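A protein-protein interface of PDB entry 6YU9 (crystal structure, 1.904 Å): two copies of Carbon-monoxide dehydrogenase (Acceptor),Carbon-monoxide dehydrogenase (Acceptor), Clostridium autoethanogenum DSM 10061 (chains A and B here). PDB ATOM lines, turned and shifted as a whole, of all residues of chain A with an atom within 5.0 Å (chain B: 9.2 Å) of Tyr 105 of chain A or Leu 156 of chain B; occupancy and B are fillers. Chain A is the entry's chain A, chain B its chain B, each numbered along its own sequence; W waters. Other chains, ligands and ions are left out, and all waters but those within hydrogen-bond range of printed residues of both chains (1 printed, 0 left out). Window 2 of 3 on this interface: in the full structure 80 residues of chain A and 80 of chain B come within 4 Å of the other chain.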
ATOM      1  N   ALA A 101     -14.807  10.927  10.559  1.00  0.00           N
ATOM      2  CA  ALA A 101     -14.323   9.825  11.398  1.00  0.00           C
ATOM      3  C   ALA A 101     -13.348   8.920  10.594  1.00  0.00           C
ATOM      4  O   ALA A 101     -12.362   8.444  11.139  1.00  0.00           O
ATOM      5  CB  ALA A 101     -15.499   9.017  11.933  1.00  0.00           C
ATOM      6  N   LEU A 102     -13.593   8.740   9.290  1.00  0.00           N
ATOM      7  CA  LEU A 102     -12.717   7.966   8.444  1.00  0.00           C
ATOM      8  C   LEU A 102     -11.351   8.696   8.308  1.00  0.00           C
ATOM      9  O   LEU A 102     -10.287   8.057   8.336  1.00  0.00           O
ATOM     10  CB  LEU A 102     -13.369   7.706   7.071  1.00  0.00           C
ATOM     11  CG  LEU A 102     -14.492   6.618   7.020  1.00  0.00           C
ATOM     12  CD1 LEU A 102     -15.298   6.694   5.726  1.00  0.00           C
ATOM     13  CD2 LEU A 102     -13.972   5.192   7.186  1.00  0.00           C
ATOM     14  N   SER A 103     -11.379  10.040   8.210  1.00  0.00           N
ATOM     15  CA  SER A 103     -10.140  10.800   8.109  1.00  0.00           C
ATOM     16  C   SER A 103      -9.342  10.667   9.411  1.00  0.00           C
ATOM     17  O   SER A 103      -8.119  10.582   9.378  1.00  0.00           O
ATOM     18  CB  SER A 103     -10.435  12.269   7.819  1.00  0.00           C
ATOM     19  OG  SER A 103     -10.697  12.512   6.445  1.00  0.00           O
ATOM     20  N   LEU A 104     -10.027  10.613  10.556  1.00  0.00           N
ATOM     21  CA  LEU A 104      -9.369  10.446  11.845  1.00  0.00           C
ATOM     22  C   LEU A 104      -8.677   9.092  11.904  1.00  0.00           C
ATOM     23  O   LEU A 104      -7.615   8.978  12.488  1.00  0.00           O
ATOM     24  CB  LEU A 104     -10.380  10.591  12.994  1.00  0.00           C
ATOM     25  CG  LEU A 104      -9.797  10.521  14.410  1.00  0.00           C
ATOM     26  CD1 LEU A 104      -8.786  11.677  14.671  1.00  0.00           C
ATOM     27  CD2 LEU A 104     -10.886  10.565  15.459  1.00  0.00           C
ATOM     28  N   TYR A 105      -9.326   8.056  11.348  1.00  0.00           N
ATOM     29  CA  TYR A 105      -8.830   6.681  11.311  1.00  0.00           C
ATOM     30  C   TYR A 105      -7.556   6.545  10.424  1.00  0.00           C
ATOM     31  O   TYR A 105      -6.806   5.577  10.560  1.00  0.00           O
ATOM     32  CB  TYR A 105      -9.915   5.769  10.749  1.00  0.00           C
ATOM     33  CG  TYR A 105      -9.536   4.307  10.772  1.00  0.00           C
ATOM     34  CD1 TYR A 105      -9.367   3.631  11.965  1.00  0.00           C
ATOM     35  CD2 TYR A 105      -9.260   3.624   9.593  1.00  0.00           C
ATOM     36  CE1 TYR A 105      -8.977   2.301  11.993  1.00  0.00           C
ATOM     37  CE2 TYR A 105      -8.901   2.287   9.606  1.00  0.00           C
ATOM     38  CZ  TYR A 105      -8.721   1.634  10.809  1.00  0.00           C
ATOM     39  OH  TYR A 105      -8.371   0.296  10.827  1.00  0.00           O
ATOM     40  N   HIS A 106      -7.352   7.470   9.484  1.00  0.00           N
ATOM     41  CA  HIS A 106      -6.213   7.436   8.581  1.00  0.00           C
ATOM     42  C   HIS A 106      -5.116   8.434   8.965  1.00  0.00           C
ATOM     43  O   HIS A 106      -4.174   8.620   8.194  1.00  0.00           O
ATOM     44  CB  HIS A 106      -6.709   7.725   7.159  1.00  0.00           C
ATOM     45  CG  HIS A 106      -7.703   6.723   6.652  1.00  0.00           C
ATOM     46  ND1 HIS A 106      -7.460   5.354   6.761  1.00  0.00           N
ATOM     47  CD2 HIS A 106      -8.881   6.910   6.010  1.00  0.00           C
ATOM     48  CE1 HIS A 106      -8.505   4.745   6.210  1.00  0.00           C
ATOM     49  NE2 HIS A 106      -9.393   5.639   5.744  1.00  0.00           N
ATOM     50  N   THR A 107      -5.206   9.057  10.153  1.00  0.00           N
ATOM     51  CA  THR A 107      -4.180  10.009  10.575  1.00  0.00           C
ATOM     52  C   THR A 107      -2.822   9.336  10.808  1.00  0.00           C
ATOM     53  O   THR A 107      -2.768   8.159  11.122  1.00  0.00           O
ATOM     54  CB  THR A 107      -4.601  10.670  11.864  1.00  0.00           C
ATOM     55  OG1 THR A 107      -4.957   9.637  12.799  1.00  0.00           O
ATOM     56  CG2 THR A 107      -5.714  11.717  11.643  1.00  0.00           C
ATOM     57  N   HIS A 142      -6.910   6.347  16.177  1.00  0.00           N
ATOM     58  CA  HIS A 142      -7.557   5.279  15.414  1.00  0.00           C
ATOM     59  C   HIS A 142      -8.585   4.546  16.233  1.00  0.00           C
ATOM     60  O   HIS A 142      -9.609   4.143  15.686  1.00  0.00           O
ATOM     61  CB  HIS A 142      -6.521   4.319  14.823  1.00  0.00           C
ATOM     62  CG  HIS A 142      -5.533   5.009  13.926  1.00  0.00           C
ATOM     63  ND1 HIS A 142      -4.325   4.419  13.600  1.00  0.00           N
ATOM     64  CD2 HIS A 142      -5.555   6.261  13.403  1.00  0.00           C
ATOM     65  CE1 HIS A 142      -3.677   5.294  12.841  1.00  0.00           C
ATOM     66  NE2 HIS A 142      -4.384   6.411  12.680  1.00  0.00           N
ATOM     67  N   ALA A 145     -11.568   6.881  16.356  1.00  0.00           N
ATOM     68  CA  ALA A 145     -12.258   6.900  15.071  1.00  0.00           C
ATOM     69  C   ALA A 145     -13.115   5.665  14.947  1.00  0.00           C
ATOM     70  O   ALA A 145     -14.254   5.783  14.514  1.00  0.00           O
ATOM     71  CB  ALA A 145     -11.274   6.925  13.916  1.00  0.00           C
ATOM     72  N   LYS A 146     -12.562   4.458  15.269  1.00  0.00           N
ATOM     73  CA  LYS A 146     -13.330   3.222  15.122  1.00  0.00           C
ATOM     74  C   LYS A 146     -14.581   3.237  15.998  1.00  0.00           C
ATOM     75  O   LYS A 146     -15.647   2.790  15.553  1.00  0.00           O
ATOM     76  CB  LYS A 146     -12.462   1.982  15.441  1.00  0.00           C
ATOM     77  CG  LYS A 146     -12.045   1.216  14.201  1.00  0.00           C
ATOM     78  CD  LYS A 146     -10.825   0.326  14.420  1.00  0.00           C
ATOM     79  CE  LYS A 146     -11.161  -0.911  15.227  1.00  0.00           C
ATOM     80  NZ  LYS A 146     -12.215  -1.760  14.576  1.00  0.00           N
ATOM     81  N   LEU A 149     -17.034   5.528  14.449  1.00  0.00           N
ATOM     82  CA  LEU A 149     -17.648   4.861  13.302  1.00  0.00           C
ATOM     83  C   LEU A 149     -18.726   3.882  13.726  1.00  0.00           C
ATOM     84  O   LEU A 149     -19.731   3.742  13.028  1.00  0.00           O
ATOM     85  CB  LEU A 149     -16.596   4.137  12.433  1.00  0.00           C
ATOM     86  CG  LEU A 149     -15.716   5.091  11.582  1.00  0.00           C
ATOM     87  CD1 LEU A 149     -14.521   4.380  11.016  1.00  0.00           C
ATOM     88  CD2 LEU A 149     -16.527   5.811  10.454  1.00  0.00           C
ATOM     89  N   SER B 150     -23.415  -7.202  10.754  1.00  0.00           N
ATOM     90  CA  SER B 150     -22.381  -6.262  10.303  1.00  0.00           C
ATOM     91  C   SER B 150     -22.560  -5.884   8.805  1.00  0.00           C
ATOM     92  O   SER B 150     -22.118  -4.807   8.379  1.00  0.00           O
ATOM     93  CB  SER B 150     -20.987  -6.810  10.559  1.00  0.00           C
ATOM     94  OG  SER B 150     -20.639  -7.738   9.546  1.00  0.00           O
ATOM     95  N   ASN B 151     -23.284  -6.705   8.037  1.00  0.00           N
ATOM     96  CA  ASN B 151     -23.617  -6.348   6.662  1.00  0.00           C
ATOM     97  C   ASN B 151     -24.592  -5.125   6.618  1.00  0.00           C
ATOM     98  O   ASN B 151     -24.655  -4.443   5.599  1.00  0.00           O
ATOM     99  CB  ASN B 151     -24.251  -7.550   5.954  1.00  0.00           C
ATOM    100  CG  ASN B 151     -23.274  -8.354   5.094  1.00  0.00           C
ATOM    101  OD1 ASN B 151     -22.093  -7.999   4.922  1.00  0.00           O
ATOM    102  ND2 ASN B 151     -23.748  -9.432   4.480  1.00  0.00           N
ATOM    103  N   GLY B 153     -24.461  -2.454   8.891  1.00  0.00           N
ATOM    104  CA  GLY B 153     -23.775  -1.235   9.314  1.00  0.00           C
ATOM    105  C   GLY B 153     -22.252  -1.182   9.389  1.00  0.00           C
ATOM    106  O   GLY B 153     -21.719  -0.244   9.997  1.00  0.00           O
ATOM    107  N   LYS B 154     -21.510  -2.125   8.811  1.00  0.00           N
ATOM    108  CA  LYS B 154     -20.039  -2.053   8.932  1.00  0.00           C
ATOM    109  C   LYS B 154     -19.519  -0.814   8.198  1.00  0.00           C
ATOM    110  O   LYS B 154     -19.984  -0.528   7.094  1.00  0.00           O
ATOM    111  CB  LYS B 154     -19.342  -3.336   8.452  1.00  0.00           C
ATOM    112  CG  LYS B 154     -19.171  -3.451   6.947  1.00  0.00           C
ATOM    113  CD  LYS B 154     -19.196  -4.884   6.443  1.00  0.00           C
ATOM    114  CE  LYS B 154     -18.209  -5.801   7.093  1.00  0.00           C
ATOM    115  NZ  LYS B 154     -18.566  -7.238   6.852  1.00  0.00           N
ATOM    116  N   GLN B 155     -18.573  -0.092   8.801  1.00  0.00           N
ATOM    117  CA  GLN B 155     -18.004   1.110   8.210  1.00  0.00           C
ATOM    118  C   GLN B 155     -16.629   0.849   7.585  1.00  0.00           C
ATOM    119  O   GLN B 155     -16.212   1.612   6.721  1.00  0.00           O
ATOM    120  CB  GLN B 155     -17.919   2.225   9.253  1.00  0.00           C
ATOM    121  CG  GLN B 155     -19.286   2.588   9.848  1.00  0.00           C
ATOM    122  CD  GLN B 155     -20.249   3.115   8.824  1.00  0.00           C
ATOM    123  OE1 GLN B 155     -19.885   3.937   7.988  1.00  0.00           O
ATOM    124  NE2 GLN B 155     -21.479   2.649   8.827  1.00  0.00           N
ATOM    125  N   LEU B 156     -15.929  -0.197   7.993  1.00  0.00           N
ATOM    126  CA  LEU B 156     -14.627  -0.505   7.399  1.00  0.00           C
ATOM    127  C   LEU B 156     -14.712  -1.929   6.895  1.00  0.00           C
ATOM    128  O   LEU B 156     -15.444  -2.718   7.479  1.00  0.00           O
ATOM    129  CB  LEU B 156     -13.493  -0.354   8.418  1.00  0.00           C
ATOM    130  CG  LEU B 156     -13.277   1.048   8.954  1.00  0.00           C
ATOM    131  CD1 LEU B 156     -12.517   1.016  10.271  1.00  0.00           C
ATOM    132  CD2 LEU B 156     -12.495   1.859   7.966  1.00  0.00           C
ATOM    133  N   GLY B 157     -13.968  -2.261   5.848  1.00  0.00           N
ATOM    134  CA  GLY B 157     -13.976  -3.627   5.343  1.00  0.00           C
ATOM    135  C   GLY B 157     -14.971  -3.869   4.230  1.00  0.00           C
ATOM    136  O   GLY B 157     -15.516  -2.926   3.663  1.00  0.00           O
ATOM    137  N   GLU B 158     -15.194  -5.126   3.888  1.00  0.00           N
ATOM    138  CA  GLU B 158     -16.052  -5.457   2.755  1.00  0.00           C
ATOM    139  C   GLU B 158     -17.271  -6.245   3.186  1.00  0.00           C
ATOM    140  O   GLU B 158     -17.203  -6.981   4.162  1.00  0.00           O
ATOM    141  CB  GLU B 158     -15.241  -6.240   1.717  1.00  0.00           C
ATOM    142  CG  GLU B 158     -14.776  -7.605   2.226  1.00  0.00           C
ATOM    143  CD  GLU B 158     -13.284  -7.799   2.443  1.00  0.00           C
ATOM    144  OE1 GLU B 158     -12.617  -6.850   2.921  1.00  0.00           O
ATOM    145  OE2 GLU B 158     -12.786  -8.917   2.166  1.00  0.00           O
ATOM    146  N   VAL B 159     -18.382  -6.093   2.485  1.00  0.00           N
ATOM    147  CA  VAL B 159     -19.586  -6.864   2.799  1.00  0.00           C
ATOM    148  C   VAL B 159     -19.432  -8.333   2.337  1.00  0.00           C
ATOM    149  O   VAL B 159     -18.586  -8.644   1.482  1.00  0.00           O
ATOM    150  CB  VAL B 159     -20.836  -6.233   2.157  1.00  0.00           C
ATOM    151  CG1 VAL B 159     -21.003  -4.779   2.626  1.00  0.00           C
ATOM    152  CG2 VAL B 159     -20.833  -6.347   0.624  1.00  0.00           C
ATOM    153  N   ARG B 181     -22.039  -1.544  -0.502  1.00  0.00           N
ATOM    154  CA  ARG B 181     -21.456  -1.305   0.824  1.00  0.00           C
ATOM    155  C   ARG B 181     -22.515  -1.740   1.856  1.00  0.00           C
ATOM    156  O   ARG B 181     -23.480  -2.479   1.490  1.00  0.00           O
ATOM    157  CB  ARG B 181     -21.035   0.173   0.995  1.00  0.00           C
ATOM    158  CG  ARG B 181     -19.940   0.599  -0.022  1.00  0.00           C
ATOM    159  CD  ARG B 181     -19.656   2.056  -0.016  1.00  0.00           C
ATOM    160  NE  ARG B 181     -20.848   2.818  -0.379  1.00  0.00           N
ATOM    161  CZ  ARG B 181     -20.888   4.140  -0.492  1.00  0.00           C
ATOM    162  NH1 ARG B 181     -19.787   4.853  -0.300  1.00  0.00           N
ATOM    163  NH2 ARG B 181     -22.012   4.755  -0.851  1.00  0.00           N
ATOM    164  N   ALA B 182     -22.362  -1.332   3.129  1.00  0.00           N
ATOM    165  CA  ALA B 182     -23.313  -1.770   4.140  1.00  0.00           C
ATOM    166  C   ALA B 182     -24.752  -1.275   3.819  1.00  0.00           C
ATOM    167  O   ALA B 182     -24.920  -0.165   3.331  1.00  0.00           O
ATOM    168  CB  ALA B 182     -22.857  -1.322   5.504  1.00  0.00           C
ATOM    169  N   ARG B 185     -25.717   2.007   5.314  1.00  0.00           N
ATOM    170  CA  ARG B 185     -24.780   3.032   4.813  1.00  0.00           C
ATOM    171  C   ARG B 185     -25.230   3.525   3.428  1.00  0.00           C
ATOM    172  O   ARG B 185     -25.135   4.709   3.143  1.00  0.00           O
ATOM    173  CB  ARG B 185     -23.385   2.414   4.692  1.00  0.00           C
ATOM    174  CG  ARG B 185     -22.272   3.387   4.472  1.00  0.00           C
ATOM    175  CD  ARG B 185     -21.999   3.632   3.024  1.00  0.00           C
ATOM    176  NE  ARG B 185     -21.142   4.811   2.849  1.00  0.00           N
ATOM    177  CZ  ARG B 185     -21.540   6.082   2.912  1.00  0.00           C
ATOM    178  NH1 ARG B 185     -20.670   7.066   2.768  1.00  0.00           N
ATOM    179  NH2 ARG B 185     -22.827   6.372   3.118  1.00  0.00           N
HETATM  180  O   HOH W   1     -20.642   0.654  12.190  1.00  0.00           O
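A ring nitrogen (NE2) of His 142 of chain A lies close to the backbone carbonyl oxygen of Tyr 105 of chain A, 3.3 Å away.
O of Gly 153 of chain B sits at hydrogen-bond distance from NE2 of Gln 155 of chain B (3.1 Å).
CD2 of Leu 102 of chain A touches CD2 of Leu 156 of chain B (3.7 Å).
Tyr 105 of chain A touches Leu 156 of chain B.
Lys 146 of chain A touches Leu 156 of chain B (CG to CD1, 3.96 Å).
Gln 155 of chain B touches Leu 149 of chain A.
CD1 of Leu 149 of chain A touches CD1 of Leu 156 of chain B, at 3.99 Å.
Of chain B, only Leu 156 comes within 4 Å of Tyr 105 of chain A.
Of the printed residues of chain A, Leu 156 of chain B touches Leu 102, Tyr 105, Lys 146 and Leu 149.
No residue of chain B comes within 4 Å of Leu 104 of chain A.
No residue of chain B comes within 4 Å of His 106 of chain A.
Printed residues of chain B within 4 Å of Lys 146 of chain A: Leu 156 (3.96 Å).
Of the printed residues of chain B, Leu 102 of chain A touches Leu 156.
Gly 153 of chain B touches none of the printed residues of chain A.
The nearest printed residue of chain B that does not touch Tyr 105 of chain A is Gly 157 of chain B (7.8 Å).
The nearest printed residue of chain A that does not touch Leu 156 of chain B is His 106 of chain A (5.2 Å).
The nearest printed residue of chain A that does not touch Gln 155 of chain B is Leu 102 of chain A (4.2 Å).
Of the 12 printed residues of chain B, 2 touch a printed residue of chain A.
Printed residues of chain B that touch a printed residue of chain A: Gln 155 and Leu 156.
Hydrophobic or aromatic side chains of chain B within 4 Å of the printed part of chain A: Leu 156.
Among the printed residues, 5 pairs touch across the chains.
Among the printed residues, no Asp or Glu carboxylate lies within 4 Å of a Lys or Arg side-chain nitrogen of the other chain.
No position is printed for both chains.
Of the 5 pairs that touch across the chains among the printed residues, none has its exchanged pair printed and touching as well.
Water W1 lies within hydrogen-bond range of O of Gly 153 of chain B (2.6 Å) and O of Leu 149 of chain A (3.3 Å).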
